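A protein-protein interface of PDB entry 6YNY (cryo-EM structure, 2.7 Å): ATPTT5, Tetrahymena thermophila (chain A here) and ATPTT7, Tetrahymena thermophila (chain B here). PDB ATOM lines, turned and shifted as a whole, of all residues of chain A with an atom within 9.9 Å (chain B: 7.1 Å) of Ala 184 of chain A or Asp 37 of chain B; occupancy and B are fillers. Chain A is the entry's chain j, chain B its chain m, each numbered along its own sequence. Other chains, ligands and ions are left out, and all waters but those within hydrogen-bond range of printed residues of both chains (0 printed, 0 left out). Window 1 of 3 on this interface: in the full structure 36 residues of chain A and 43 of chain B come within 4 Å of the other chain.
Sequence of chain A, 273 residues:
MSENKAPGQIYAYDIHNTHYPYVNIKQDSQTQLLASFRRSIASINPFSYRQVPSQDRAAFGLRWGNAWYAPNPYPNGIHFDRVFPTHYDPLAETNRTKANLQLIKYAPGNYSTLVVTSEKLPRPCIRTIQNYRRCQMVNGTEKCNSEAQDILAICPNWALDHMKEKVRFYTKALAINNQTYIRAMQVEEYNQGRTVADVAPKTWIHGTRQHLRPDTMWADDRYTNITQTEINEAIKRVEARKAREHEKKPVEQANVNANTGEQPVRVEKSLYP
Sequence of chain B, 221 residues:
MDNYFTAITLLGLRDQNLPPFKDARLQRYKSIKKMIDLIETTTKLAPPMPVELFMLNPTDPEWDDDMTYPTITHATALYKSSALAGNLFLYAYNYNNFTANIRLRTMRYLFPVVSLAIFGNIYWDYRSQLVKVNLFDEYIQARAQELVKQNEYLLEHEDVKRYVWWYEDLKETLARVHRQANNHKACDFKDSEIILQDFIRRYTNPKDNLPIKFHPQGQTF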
ATOM      1  N   ILE A 176      17.694  12.121   3.437  1.00  0.00           N
ATOM      2  CA  ILE A 176      18.888  11.329   3.703  1.00  0.00           C
ATOM      3  C   ILE A 176      19.820  12.068   4.650  1.00  0.00           C
ATOM      4  O   ILE A 176      20.465  11.457   5.510  1.00  0.00           O
ATOM      5  CB  ILE A 176      19.578  10.964   2.379  1.00  0.00           C
ATOM      6  CG1 ILE A 176      18.761   9.896   1.656  1.00  0.00           C
ATOM      7  CG2 ILE A 176      20.996  10.489   2.623  1.00  0.00           C
ATOM      8  CD1 ILE A 176      19.170   9.656   0.239  1.00  0.00           C
ATOM      9  N   ASN A 177      19.908  13.390   4.514  1.00  0.00           N
ATOM     10  CA  ASN A 177      20.741  14.164   5.422  1.00  0.00           C
ATOM     11  C   ASN A 177      20.113  14.283   6.804  1.00  0.00           C
ATOM     12  O   ASN A 177      20.833  14.413   7.799  1.00  0.00           O
ATOM     13  CB  ASN A 177      21.005  15.548   4.836  1.00  0.00           C
ATOM     14  CG  ASN A 177      22.000  15.517   3.699  1.00  0.00           C
ATOM     15  OD1 ASN A 177      22.896  14.677   3.666  1.00  0.00           O
ATOM     16  ND2 ASN A 177      21.850  16.435   2.758  1.00  0.00           N
ATOM     17  N   ASN A 178      18.783  14.241   6.889  1.00  0.00           N
ATOM     18  CA  ASN A 178      18.122  14.315   8.185  1.00  0.00           C
ATOM     19  C   ASN A 178      18.106  12.970   8.898  1.00  0.00           C
ATOM     20  O   ASN A 178      18.134  12.930  10.132  1.00  0.00           O
ATOM     21  CB  ASN A 178      16.699  14.846   8.022  1.00  0.00           C
ATOM     22  CG  ASN A 178      16.645  16.357   7.991  1.00  0.00           C
ATOM     23  OD1 ASN A 178      16.562  17.007   9.030  1.00  0.00           O
ATOM     24  ND2 ASN A 178      16.690  16.925   6.798  1.00  0.00           N
ATOM     25  N   GLN A 179      18.058  11.865   8.154  1.00  0.00           N
ATOM     26  CA  GLN A 179      18.222  10.559   8.779  1.00  0.00           C
ATOM     27  C   GLN A 179      19.617  10.413   9.369  1.00  0.00           C
ATOM     28  O   GLN A 179      19.784   9.876  10.469  1.00  0.00           O
ATOM     29  CB  GLN A 179      17.960   9.448   7.766  1.00  0.00           C
ATOM     30  CG  GLN A 179      16.513   9.278   7.374  1.00  0.00           C
ATOM     31  CD  GLN A 179      16.295   8.051   6.519  1.00  0.00           C
ATOM     32  OE1 GLN A 179      17.246   7.441   6.035  1.00  0.00           O
ATOM     33  NE2 GLN A 179      15.040   7.674   6.338  1.00  0.00           N
ATOM     34  N   THR A 180      20.632  10.882   8.644  1.00  0.00           N
ATOM     35  CA  THR A 180      21.985  10.900   9.183  1.00  0.00           C
ATOM     36  C   THR A 180      22.065  11.786  10.418  1.00  0.00           C
ATOM     37  O   THR A 180      22.791  11.478  11.370  1.00  0.00           O
ATOM     38  CB  THR A 180      22.957  11.383   8.108  1.00  0.00           C
ATOM     39  OG1 THR A 180      22.780  10.604   6.920  1.00  0.00           O
ATOM     40  CG2 THR A 180      24.389  11.255   8.568  1.00  0.00           C
ATOM     41  N   TYR A 181      21.320  12.891  10.420  1.00  0.00           N
ATOM     42  CA  TYR A 181      21.264  13.760  11.588  1.00  0.00           C
ATOM     43  C   TYR A 181      20.729  13.012  12.801  1.00  0.00           C
ATOM     44  O   TYR A 181      21.252  13.155  13.911  1.00  0.00           O
ATOM     45  CB  TYR A 181      20.390  14.971  11.275  1.00  0.00           C
ATOM     46  CG  TYR A 181      20.327  16.024  12.354  1.00  0.00           C
ATOM     47  CD1 TYR A 181      21.109  17.161  12.277  1.00  0.00           C
ATOM     48  CD2 TYR A 181      19.472  15.893  13.435  1.00  0.00           C
ATOM     49  CE1 TYR A 181      21.051  18.130  13.246  1.00  0.00           C
ATOM     50  CE2 TYR A 181      19.410  16.859  14.411  1.00  0.00           C
ATOM     51  CZ  TYR A 181      20.203  17.975  14.313  1.00  0.00           C
ATOM     52  OH  TYR A 181      20.151  18.949  15.278  1.00  0.00           O
ATOM     53  N   ILE A 182      19.690  12.204  12.604  1.00  0.00           N
ATOM     54  CA  ILE A 182      19.075  11.488  13.714  1.00  0.00           C
ATOM     55  C   ILE A 182      20.039  10.461  14.289  1.00  0.00           C
ATOM     56  O   ILE A 182      20.261  10.406  15.503  1.00  0.00           O
ATOM     57  CB  ILE A 182      17.760  10.838  13.254  1.00  0.00           C
ATOM     58  CG1 ILE A 182      16.745  11.922  12.908  1.00  0.00           C
ATOM     59  CG2 ILE A 182      17.216   9.927  14.324  1.00  0.00           C
ATOM     60  CD1 ILE A 182      15.596  11.434  12.083  1.00  0.00           C
ATOM     61  N   ARG A 183      20.624   9.626  13.428  1.00  0.00           N
ATOM     62  CA  ARG A 183      21.571   8.629  13.910  1.00  0.00           C
ATOM     63  C   ARG A 183      22.770   9.280  14.581  1.00  0.00           C
ATOM     64  O   ARG A 183      23.384   8.683  15.471  1.00  0.00           O
ATOM     65  CB  ARG A 183      22.030   7.737  12.761  1.00  0.00           C
ATOM     66  CG  ARG A 183      20.930   6.897  12.150  1.00  0.00           C
ATOM     67  CD  ARG A 183      21.501   5.873  11.196  1.00  0.00           C
ATOM     68  NE  ARG A 183      22.321   6.496  10.163  1.00  0.00           N
ATOM     69  CZ  ARG A 183      21.873   6.880   8.974  1.00  0.00           C
ATOM     70  NH1 ARG A 183      20.601   6.708   8.640  1.00  0.00           N
ATOM     71  NH2 ARG A 183      22.705   7.441   8.114  1.00  0.00           N
ATOM     72  N   ALA A 184      23.116  10.497  14.170  1.00  0.00           N
ATOM     73  CA  ALA A 184      24.259  11.185  14.752  1.00  0.00           C
ATOM     74  C   ALA A 184      23.929  11.760  16.120  1.00  0.00           C
ATOM     75  O   ALA A 184      24.731  11.647  17.053  1.00  0.00           O
ATOM     76  CB  ALA A 184      24.727  12.290  13.815  1.00  0.00           C
ATOM     77  N   MET A 185      22.764  12.381  16.256  1.00  0.00           N
ATOM     78  CA  MET A 185      22.349  12.995  17.507  1.00  0.00           C
ATOM     79  C   MET A 185      21.707  12.005  18.464  1.00  0.00           C
ATOM     80  O   MET A 185      21.202  12.414  19.513  1.00  0.00           O
ATOM     81  CB  MET A 185      21.382  14.141  17.219  1.00  0.00           C
ATOM     82  CG  MET A 185      21.934  15.156  16.250  1.00  0.00           C
ATOM     83  SD  MET A 185      23.414  15.985  16.840  1.00  0.00           S
ATOM     84  CE  MET A 185      22.727  16.915  18.195  1.00  0.00           C
ATOM     85  N   GLN A 186      21.711  10.721  18.128  1.00  0.00           N
ATOM     86  CA  GLN A 186      21.173   9.713  19.027  1.00  0.00           C
ATOM     87  C   GLN A 186      22.120   9.503  20.197  1.00  0.00           C
ATOM     88  O   GLN A 186      23.334   9.374  20.014  1.00  0.00           O
ATOM     89  CB  GLN A 186      20.961   8.400  18.281  1.00  0.00           C
ATOM     90  CG  GLN A 186      19.668   7.701  18.612  1.00  0.00           C
ATOM     91  CD  GLN A 186      19.561   6.343  17.952  1.00  0.00           C
ATOM     92  OE1 GLN A 186      20.479   5.905  17.260  1.00  0.00           O
ATOM     93  NE2 GLN A 186      18.441   5.666  18.168  1.00  0.00           N
ATOM     94  N   VAL A 187      21.564   9.475  21.401  1.00  0.00           N
ATOM     95  CA  VAL A 187      22.346   9.313  22.618  1.00  0.00           C
ATOM     96  C   VAL A 187      22.422   7.830  22.942  1.00  0.00           C
ATOM     97  O   VAL A 187      21.399   7.189  23.208  1.00  0.00           O
ATOM     98  CB  VAL A 187      21.738  10.104  23.783  1.00  0.00           C
ATOM     99  CG1 VAL A 187      22.547   9.890  25.036  1.00  0.00           C
ATOM    100  CG2 VAL A 187      21.676  11.578  23.439  1.00  0.00           C
ATOM    101  N   GLU A 188      23.632   7.282  22.920  1.00  0.00           N
ATOM    102  CA  GLU A 188      23.818   5.867  23.176  1.00  0.00           C
ATOM    103  C   GLU A 188      23.746   5.583  24.674  1.00  0.00           C
ATOM    104  O   GLU A 188      23.805   6.483  25.514  1.00  0.00           O
ATOM    105  CB  GLU A 188      25.152   5.398  22.604  1.00  0.00           C
ATOM    106  CG  GLU A 188      25.366   5.763  21.145  1.00  0.00           C
ATOM    107  CD  GLU A 188      24.333   5.153  20.222  1.00  0.00           C
ATOM    108  OE1 GLU A 188      23.576   4.269  20.672  1.00  0.00           O
ATOM    109  OE2 GLU A 188      24.279   5.559  19.043  1.00  0.00           O
ATOM    110  N   TYR A 190      25.884   4.343  26.580  1.00  0.00           N
ATOM    111  CA  TYR A 190      27.119   4.654  27.285  1.00  0.00           C
ATOM    112  C   TYR A 190      27.351   6.148  27.456  1.00  0.00           C
ATOM    113  O   TYR A 190      28.377   6.537  28.021  1.00  0.00           O
ATOM    114  CB  TYR A 190      28.318   4.028  26.563  1.00  0.00           C
ATOM    115  CG  TYR A 190      28.421   4.369  25.096  1.00  0.00           C
ATOM    116  CD1 TYR A 190      28.969   5.571  24.677  1.00  0.00           C
ATOM    117  CD2 TYR A 190      27.982   3.480  24.127  1.00  0.00           C
ATOM    118  CE1 TYR A 190      29.068   5.882  23.340  1.00  0.00           C
ATOM    119  CE2 TYR A 190      28.076   3.783  22.788  1.00  0.00           C
ATOM    120  CZ  TYR A 190      28.621   4.984  22.399  1.00  0.00           C
ATOM    121  OH  TYR A 190      28.718   5.293  21.062  1.00  0.00           O
ATOM    122  N   ASN A 191      26.432   6.993  26.985  1.00  0.00           N
ATOM    123  CA  ASN A 191      26.543   8.436  27.160  1.00  0.00           C
ATOM    124  C   ASN A 191      25.284   9.037  27.775  1.00  0.00           C
ATOM    125  O   ASN A 191      25.061  10.246  27.658  1.00  0.00           O
ATOM    126  CB  ASN A 191      26.863   9.122  25.831  1.00  0.00           C
ATOM    127  CG  ASN A 191      28.349   9.329  25.626  1.00  0.00           C
ATOM    128  OD1 ASN A 191      29.127   9.324  26.577  1.00  0.00           O
ATOM    129  ND2 ASN A 191      28.748   9.529  24.379  1.00  0.00           N
ATOM    130  N   ILE B  32      33.793   3.503  13.914  1.00  0.00           N
ATOM    131  CA  ILE B  32      33.776   4.899  13.492  1.00  0.00           C
ATOM    132  C   ILE B  32      32.465   5.216  12.789  1.00  0.00           C
ATOM    133  O   ILE B  32      32.285   6.314  12.252  1.00  0.00           O
ATOM    134  CB  ILE B  32      34.974   5.209  12.579  1.00  0.00           C
ATOM    135  CG1 ILE B  32      34.972   4.281  11.363  1.00  0.00           C
ATOM    136  CG2 ILE B  32      36.260   5.062  13.354  1.00  0.00           C
ATOM    137  CD1 ILE B  32      36.016   4.611  10.346  1.00  0.00           C
ATOM    138  N   LYS B  33      31.537   4.261  12.794  1.00  0.00           N
ATOM    139  CA  LYS B  33      30.275   4.452  12.091  1.00  0.00           C
ATOM    140  C   LYS B  33      29.496   5.633  12.654  1.00  0.00           C
ATOM    141  O   LYS B  33      28.888   6.402  11.902  1.00  0.00           O
ATOM    142  CB  LYS B  33      29.453   3.172  12.177  1.00  0.00           C
ATOM    143  CG  LYS B  33      28.340   3.067  11.173  1.00  0.00           C
ATOM    144  CD  LYS B  33      27.711   1.691  11.221  1.00  0.00           C
ATOM    145  CE  LYS B  33      28.574   0.660  10.519  1.00  0.00           C
ATOM    146  NZ  LYS B  33      28.119  -0.724  10.789  1.00  0.00           N
ATOM    147  N   LYS B  34      29.504   5.794  13.977  1.00  0.00           N
ATOM    148  CA  LYS B  34      28.806   6.916  14.591  1.00  0.00           C
ATOM    149  C   LYS B  34      29.498   8.233  14.282  1.00  0.00           C
ATOM    150  O   LYS B  34      28.836   9.250  14.041  1.00  0.00           O
ATOM    151  CB  LYS B  34      28.724   6.700  16.100  1.00  0.00           C
ATOM    152  CG  LYS B  34      28.076   7.827  16.885  1.00  0.00           C
ATOM    153  CD  LYS B  34      26.583   7.832  16.729  1.00  0.00           C
ATOM    154  CE  LYS B  34      25.938   8.740  17.748  1.00  0.00           C
ATOM    155  NZ  LYS B  34      24.477   8.518  17.833  1.00  0.00           N
ATOM    156  N   MET B  35      30.830   8.236  14.286  1.00  0.00           N
ATOM    157  CA  MET B  35      31.568   9.479  14.106  1.00  0.00           C
ATOM    158  C   MET B  35      31.468   9.999  12.681  1.00  0.00           C
ATOM    159  O   MET B  35      31.454  11.216  12.468  1.00  0.00           O
ATOM    160  CB  MET B  35      33.027   9.267  14.492  1.00  0.00           C
ATOM    161  CG  MET B  35      33.216   8.779  15.912  1.00  0.00           C
ATOM    162  SD  MET B  35      32.516   9.890  17.140  1.00  0.00           S
ATOM    163  CE  MET B  35      33.384  11.395  16.737  1.00  0.00           C
ATOM    164  N   ILE B  36      31.405   9.104  11.695  1.00  0.00           N
ATOM    165  CA  ILE B  36      31.281   9.543  10.310  1.00  0.00           C
ATOM    166  C   ILE B  36      29.952  10.253  10.098  1.00  0.00           C
ATOM    167  O   ILE B  36      29.877  11.269   9.398  1.00  0.00           O
ATOM    168  CB  ILE B  36      31.444   8.348   9.356  1.00  0.00           C
ATOM    169  CG1 ILE B  36      32.837   7.739   9.489  1.00  0.00           C
ATOM    170  CG2 ILE B  36      31.200   8.780   7.929  1.00  0.00           C
ATOM    171  CD1 ILE B  36      33.940   8.586   8.939  1.00  0.00           C
ATOM    172  N   ASP B  37      28.880   9.732  10.697  1.00  0.00           N
ATOM    173  CA  ASP B  37      27.585  10.390  10.590  1.00  0.00           C
ATOM    174  C   ASP B  37      27.589  11.748  11.273  1.00  0.00           C
ATOM    175  O   ASP B  37      26.842  12.646  10.868  1.00  0.00           O
ATOM    176  CB  ASP B  37      26.493   9.502  11.181  1.00  0.00           C
ATOM    177  CG  ASP B  37      26.252   8.251  10.362  1.00  0.00           C
ATOM    178  OD1 ASP B  37      27.153   7.391  10.305  1.00  0.00           O
ATOM    179  OD2 ASP B  37      25.159   8.127   9.772  1.00  0.00           O
ATOM    180  N   LEU B  38      28.412  11.919  12.305  1.00  0.00           N
ATOM    181  CA  LEU B  38      28.509  13.207  12.975  1.00  0.00           C
ATOM    182  C   LEU B  38      29.331  14.191  12.158  1.00  0.00           C
ATOM    183  O   LEU B  38      28.893  15.317  11.904  1.00  0.00           O
ATOM    184  CB  LEU B  38      29.124  13.024  14.358  1.00  0.00           C
ATOM    185  CG  LEU B  38      28.174  12.577  15.463  1.00  0.00           C
ATOM    186  CD1 LEU B  38      28.940  11.971  16.602  1.00  0.00           C
ATOM    187  CD2 LEU B  38      27.359  13.748  15.954  1.00  0.00           C
ATOM    188  N   ILE B  39      30.525  13.778  11.736  1.00  0.00           N
ATOM    189  CA  ILE B  39      31.385  14.663  10.961  1.00  0.00           C
ATOM    190  C   ILE B  39      30.744  14.998   9.625  1.00  0.00           C
ATOM    191  O   ILE B  39      30.954  16.088   9.082  1.00  0.00           O
ATOM    192  CB  ILE B  39      32.772  14.018  10.794  1.00  0.00           C
ATOM    193  CG1 ILE B  39      33.419  13.834  12.165  1.00  0.00           C
ATOM    194  CG2 ILE B  39      33.647  14.864   9.908  1.00  0.00           C
ATOM    195  CD1 ILE B  39      34.700  13.067  12.149  1.00  0.00           C
ATOM    196  N   GLU B  40      29.952  14.079   9.073  1.00  0.00           N
ATOM    197  CA  GLU B  40      29.207  14.385   7.858  1.00  0.00           C
ATOM    198  C   GLU B  40      28.162  15.461   8.111  1.00  0.00           C
ATOM    199  O   GLU B  40      27.952  16.340   7.268  1.00  0.00           O
ATOM    200  CB  GLU B  40      28.543  13.123   7.318  1.00  0.00           C
ATOM    201  CG  GLU B  40      29.472  12.214   6.547  1.00  0.00           C
ATOM    202  CD  GLU B  40      28.786  10.947   6.077  1.00  0.00           C
ATOM    203  OE1 GLU B  40      27.693  10.633   6.590  1.00  0.00           O
ATOM    204  OE2 GLU B  40      29.336  10.266   5.186  1.00  0.00           O
ATOM    205  N   THR B  41      27.494  15.406   9.264  1.00  0.00           N
ATOM    206  CA  THR B  41      26.464  16.391   9.564  1.00  0.00           C
ATOM    207  C   THR B  41      27.073  17.759   9.836  1.00  0.00           C
ATOM    208  O   THR B  41      26.522  18.782   9.417  1.00  0.00           O
ATOM    209  CB  THR B  41      25.631  15.929  10.757  1.00  0.00           C
ATOM    210  OG1 THR B  41      25.075  14.639  10.482  1.00  0.00           O
ATOM    211  CG2 THR B  41      24.512  16.904  11.031  1.00  0.00           C
ATOM    212  N   THR B  42      28.205  17.800  10.537  1.00  0.00           N
ATOM    213  CA  THR B  42      28.858  19.077  10.803  1.00  0.00           C
ATOM    214  C   THR B  42      29.176  19.809   9.508  1.00  0.00           C
ATOM    215  O   THR B  42      29.084  21.039   9.440  1.00  0.00           O
ATOM    216  CB  THR B  42      30.136  18.860  11.612  1.00  0.00           C
ATOM    217  OG1 THR B  42      31.028  18.006  10.887  1.00  0.00           O
ATOM    218  CG2 THR B  42      29.823  18.236  12.947  1.00  0.00           C
ATOM    219  N   LYS B  44      27.507  19.948   6.871  1.00  0.00           N
ATOM    220  CA  LYS B  44      26.303  20.397   6.186  1.00  0.00           C
ATOM    221  C   LYS B  44      25.603  21.522   6.934  1.00  0.00           C
ATOM    222  O   LYS B  44      24.400  21.730   6.752  1.00  0.00           O
ATOM    223  CB  LYS B  44      25.351  19.220   5.987  1.00  0.00           C
ATOM    224  CG  LYS B  44      25.901  18.144   5.078  1.00  0.00           C
ATOM    225  CD  LYS B  44      25.129  16.865   5.215  1.00  0.00           C
ATOM    226  CE  LYS B  44      25.774  15.750   4.415  1.00  0.00           C
ATOM    227  NZ  LYS B  44      25.140  14.429   4.700  1.00  0.00           N
ATOM    228  N   GLU B 193      31.629  12.283  20.791  1.00  0.00           N
ATOM    229  CA  GLU B 193      30.245  12.407  20.353  1.00  0.00           C
ATOM    230  C   GLU B 193      29.575  13.601  21.013  1.00  0.00           C
ATOM    231  O   GLU B 193      28.774  14.303  20.386  1.00  0.00           O
ATOM    232  CB  GLU B 193      29.476  11.128  20.673  1.00  0.00           C
ATOM    233  CG  GLU B 193      30.000   9.889  19.984  1.00  0.00           C
ATOM    234  CD  GLU B 193      29.246   8.643  20.388  1.00  0.00           C
ATOM    235  OE1 GLU B 193      28.175   8.774  21.016  1.00  0.00           O
ATOM    236  OE2 GLU B 193      29.725   7.530  20.084  1.00  0.00           O
ATOM    237  N   GLN B 197      28.072  16.741  18.997  1.00  0.00           N
ATOM    238  CA  GLN B 197      26.655  16.998  19.225  1.00  0.00           C
ATOM    239  C   GLN B 197      26.422  18.430  19.685  1.00  0.00           C
ATOM    240  O   GLN B 197      25.415  19.048  19.325  1.00  0.00           O
ATOM    241  CB  GLN B 197      26.103  16.011  20.247  1.00  0.00           C
ATOM    242  CG  GLN B 197      25.882  14.625  19.697  1.00  0.00           C
ATOM    243  CD  GLN B 197      25.460  13.636  20.754  1.00  0.00           C
ATOM    244  OE1 GLN B 197      25.361  13.972  21.933  1.00  0.00           O
ATOM    245  NE2 GLN B 197      25.208  12.404  20.338  1.00  0.00           N
ATOM    246  N   ILE B 200      26.644  20.542  16.551  1.00  0.00           N
ATOM    247  CA  ILE B 200      25.443  20.439  15.732  1.00  0.00           C
ATOM    248  C   ILE B 200      24.285  21.161  16.401  1.00  0.00           C
ATOM    249  O   ILE B 200      23.547  21.916  15.760  1.00  0.00           O
ATOM    250  CB  ILE B 200      25.110  18.962  15.466  1.00  0.00           C
ATOM    251  CG1 ILE B 200      26.276  18.276  14.756  1.00  0.00           C
ATOM    252  CG2 ILE B 200      23.864  18.845  14.625  1.00  0.00           C
ATOM    253  CD1 ILE B 200      26.160  16.779  14.698  1.00  0.00           C
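The side-chain amide oxygen (OD1) of Asn 177 of chain A lies within hydrogen-bond range of the side-chain amino group (NZ) of Lys 44 of chain B (2.5 Å).
The side-chain amino group of Lys 34 of chain B sits at hydrogen-bond distance from the backbone carbonyl oxygen of Arg 183 of chain A, 2.6 Å away.
NH2 of Arg 183 of chain A is in salt-bridge range of OD2 of Asp 37 of chain B (3.0 Å).
The backbone carbonyl oxygen of Ala 184 of chain A lies close to the side-chain amino group of Lys 34 of chain B (3.2 Å).
The side-chain amide nitrogen (NE2) of Gln 197 of chain B lies within hydrogen-bond range of the backbone carbonyl oxygen (O) of Ala 184 of chain A, 3.4 Å away.
The backbone carbonyl oxygen (O) of Gln 186 of chain A is in hydrogen-bond range of the side-chain amino group (NZ) of Lys 34 of chain B (2.6 Å).
OE2 of Glu 188 of chain A lies within salt-bridge range of NZ of Lys 34 of chain B (3.2 Å).
OE2 of Glu 193 of chain B is in hydrogen-bond range of OH of Tyr 190 of chain A (2.6 Å).
The side-chain amide nitrogen of Asn 191 of chain A is in hydrogen-bond range of the side-chain carboxylate of Glu 193 of chain B, at 3.5 Å.
The side-chain hydroxyl (OG1) of Thr 180 of chain A is in hydrogen-bond range of the backbone carbonyl oxygen (O) of Ile 176 of chain A (2.8 Å).
The guanidinium group (NH2) of Arg 183 of chain A sits at hydrogen-bond distance from the side-chain hydroxyl (OG1) of Thr 180 of chain A, 3.4 Å away.
The side-chain carboxylate (OD1) of Asp 37 of chain B sits close to the backbone carbonyl oxygen (O) of Lys 33 of chain B.
The side-chain hydroxyl (OG1) of Thr 41 of chain B lies within hydrogen-bond range of the backbone carbonyl oxygen (O) of Asp 37 of chain B (2.7 Å).
Of the printed residues of chain B, Ala 184 of chain A touches Lys 34, Asp 37, Leu 38 and Gln 197.
Printed residues of chain B within 4 Å of Asn 191 of chain A: Glu 193 (3.5 Å).
No residue of chain A comes within 4 Å of Ile 36 of chain B.
Printed residues of chain A within 4 Å of Asp 37 of chain B: Thr 180, Arg 183 and Ala 184.
Of the printed residues of chain A, Leu 38 of chain B touches Ala 184 (3.5 Å).
Glu 40 of chain B touches one residue of chain A.
Of the printed residues of chain A, Lys 44 of chain B touches Asn 177 (2.5 Å).
Of the printed residues of chain A, Gln 197 of chain B touches Ala 184 (3.4 Å), Met 185 (3.6 Å) and Gln 186 (3.6 Å).
The nearest residue of chain B that does not touch Ala 184 of chain A is Thr 41 of chain B (4.1 Å).
The nearest residue of chain A that does not touch Asp 37 of chain B is Tyr 181 of chain A (5.5 Å).
Hydrophobic or aromatic side chains of chain B that line the printed part of chain A: Leu 38 and Ile 200.
Printed residues of chain A that touch a printed residue of chain B: Asn 177, Thr 180, Tyr 181, Arg 183, Ala 184, Met 185, Gln 186, Glu 188, Tyr 190 and Asn 191.
Among the printed residues, 19 pairs touch across the chains.
Among the printed residues, Asp or Glu carboxylates within 4 Å of a Lys or Arg side-chain nitrogen of the other chain: Arg 183 of chain A with Asp 37 of chain B (3.0 Å) and Glu 188 of chain A with Lys 34 of chain B (3.2 Å).
CG2 of Thr 180 of chain A touches OD2 of Asp 37 of chain B (3.4 Å).
Glu 40 of chain B touches Thr 180 of chain A (OE1 to CG2, 3.9 Å).
Thr 180 of chain A touches Thr 41 of chain B.
CD1 of Tyr 181 of chain A touches CG2 of Thr 41 of chain B, 3.6 Å away.
Ile 200 of chain B touches Tyr 181 of chain A (CG2 to CE1, 3.2 Å).
Ala 184 of chain A touches Asp 37 of chain B.
Ala 184 of chain A touches Leu 38 of chain B.
Gln 197 of chain B touches Met 185 of chain A.
Met 185 of chain A touches Ile 200 of chain B (SD to CD1, 3.6 Å).
Gln 197 of chain B touches Gln 186 of chain A (NE2 to O, 3.6 Å).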
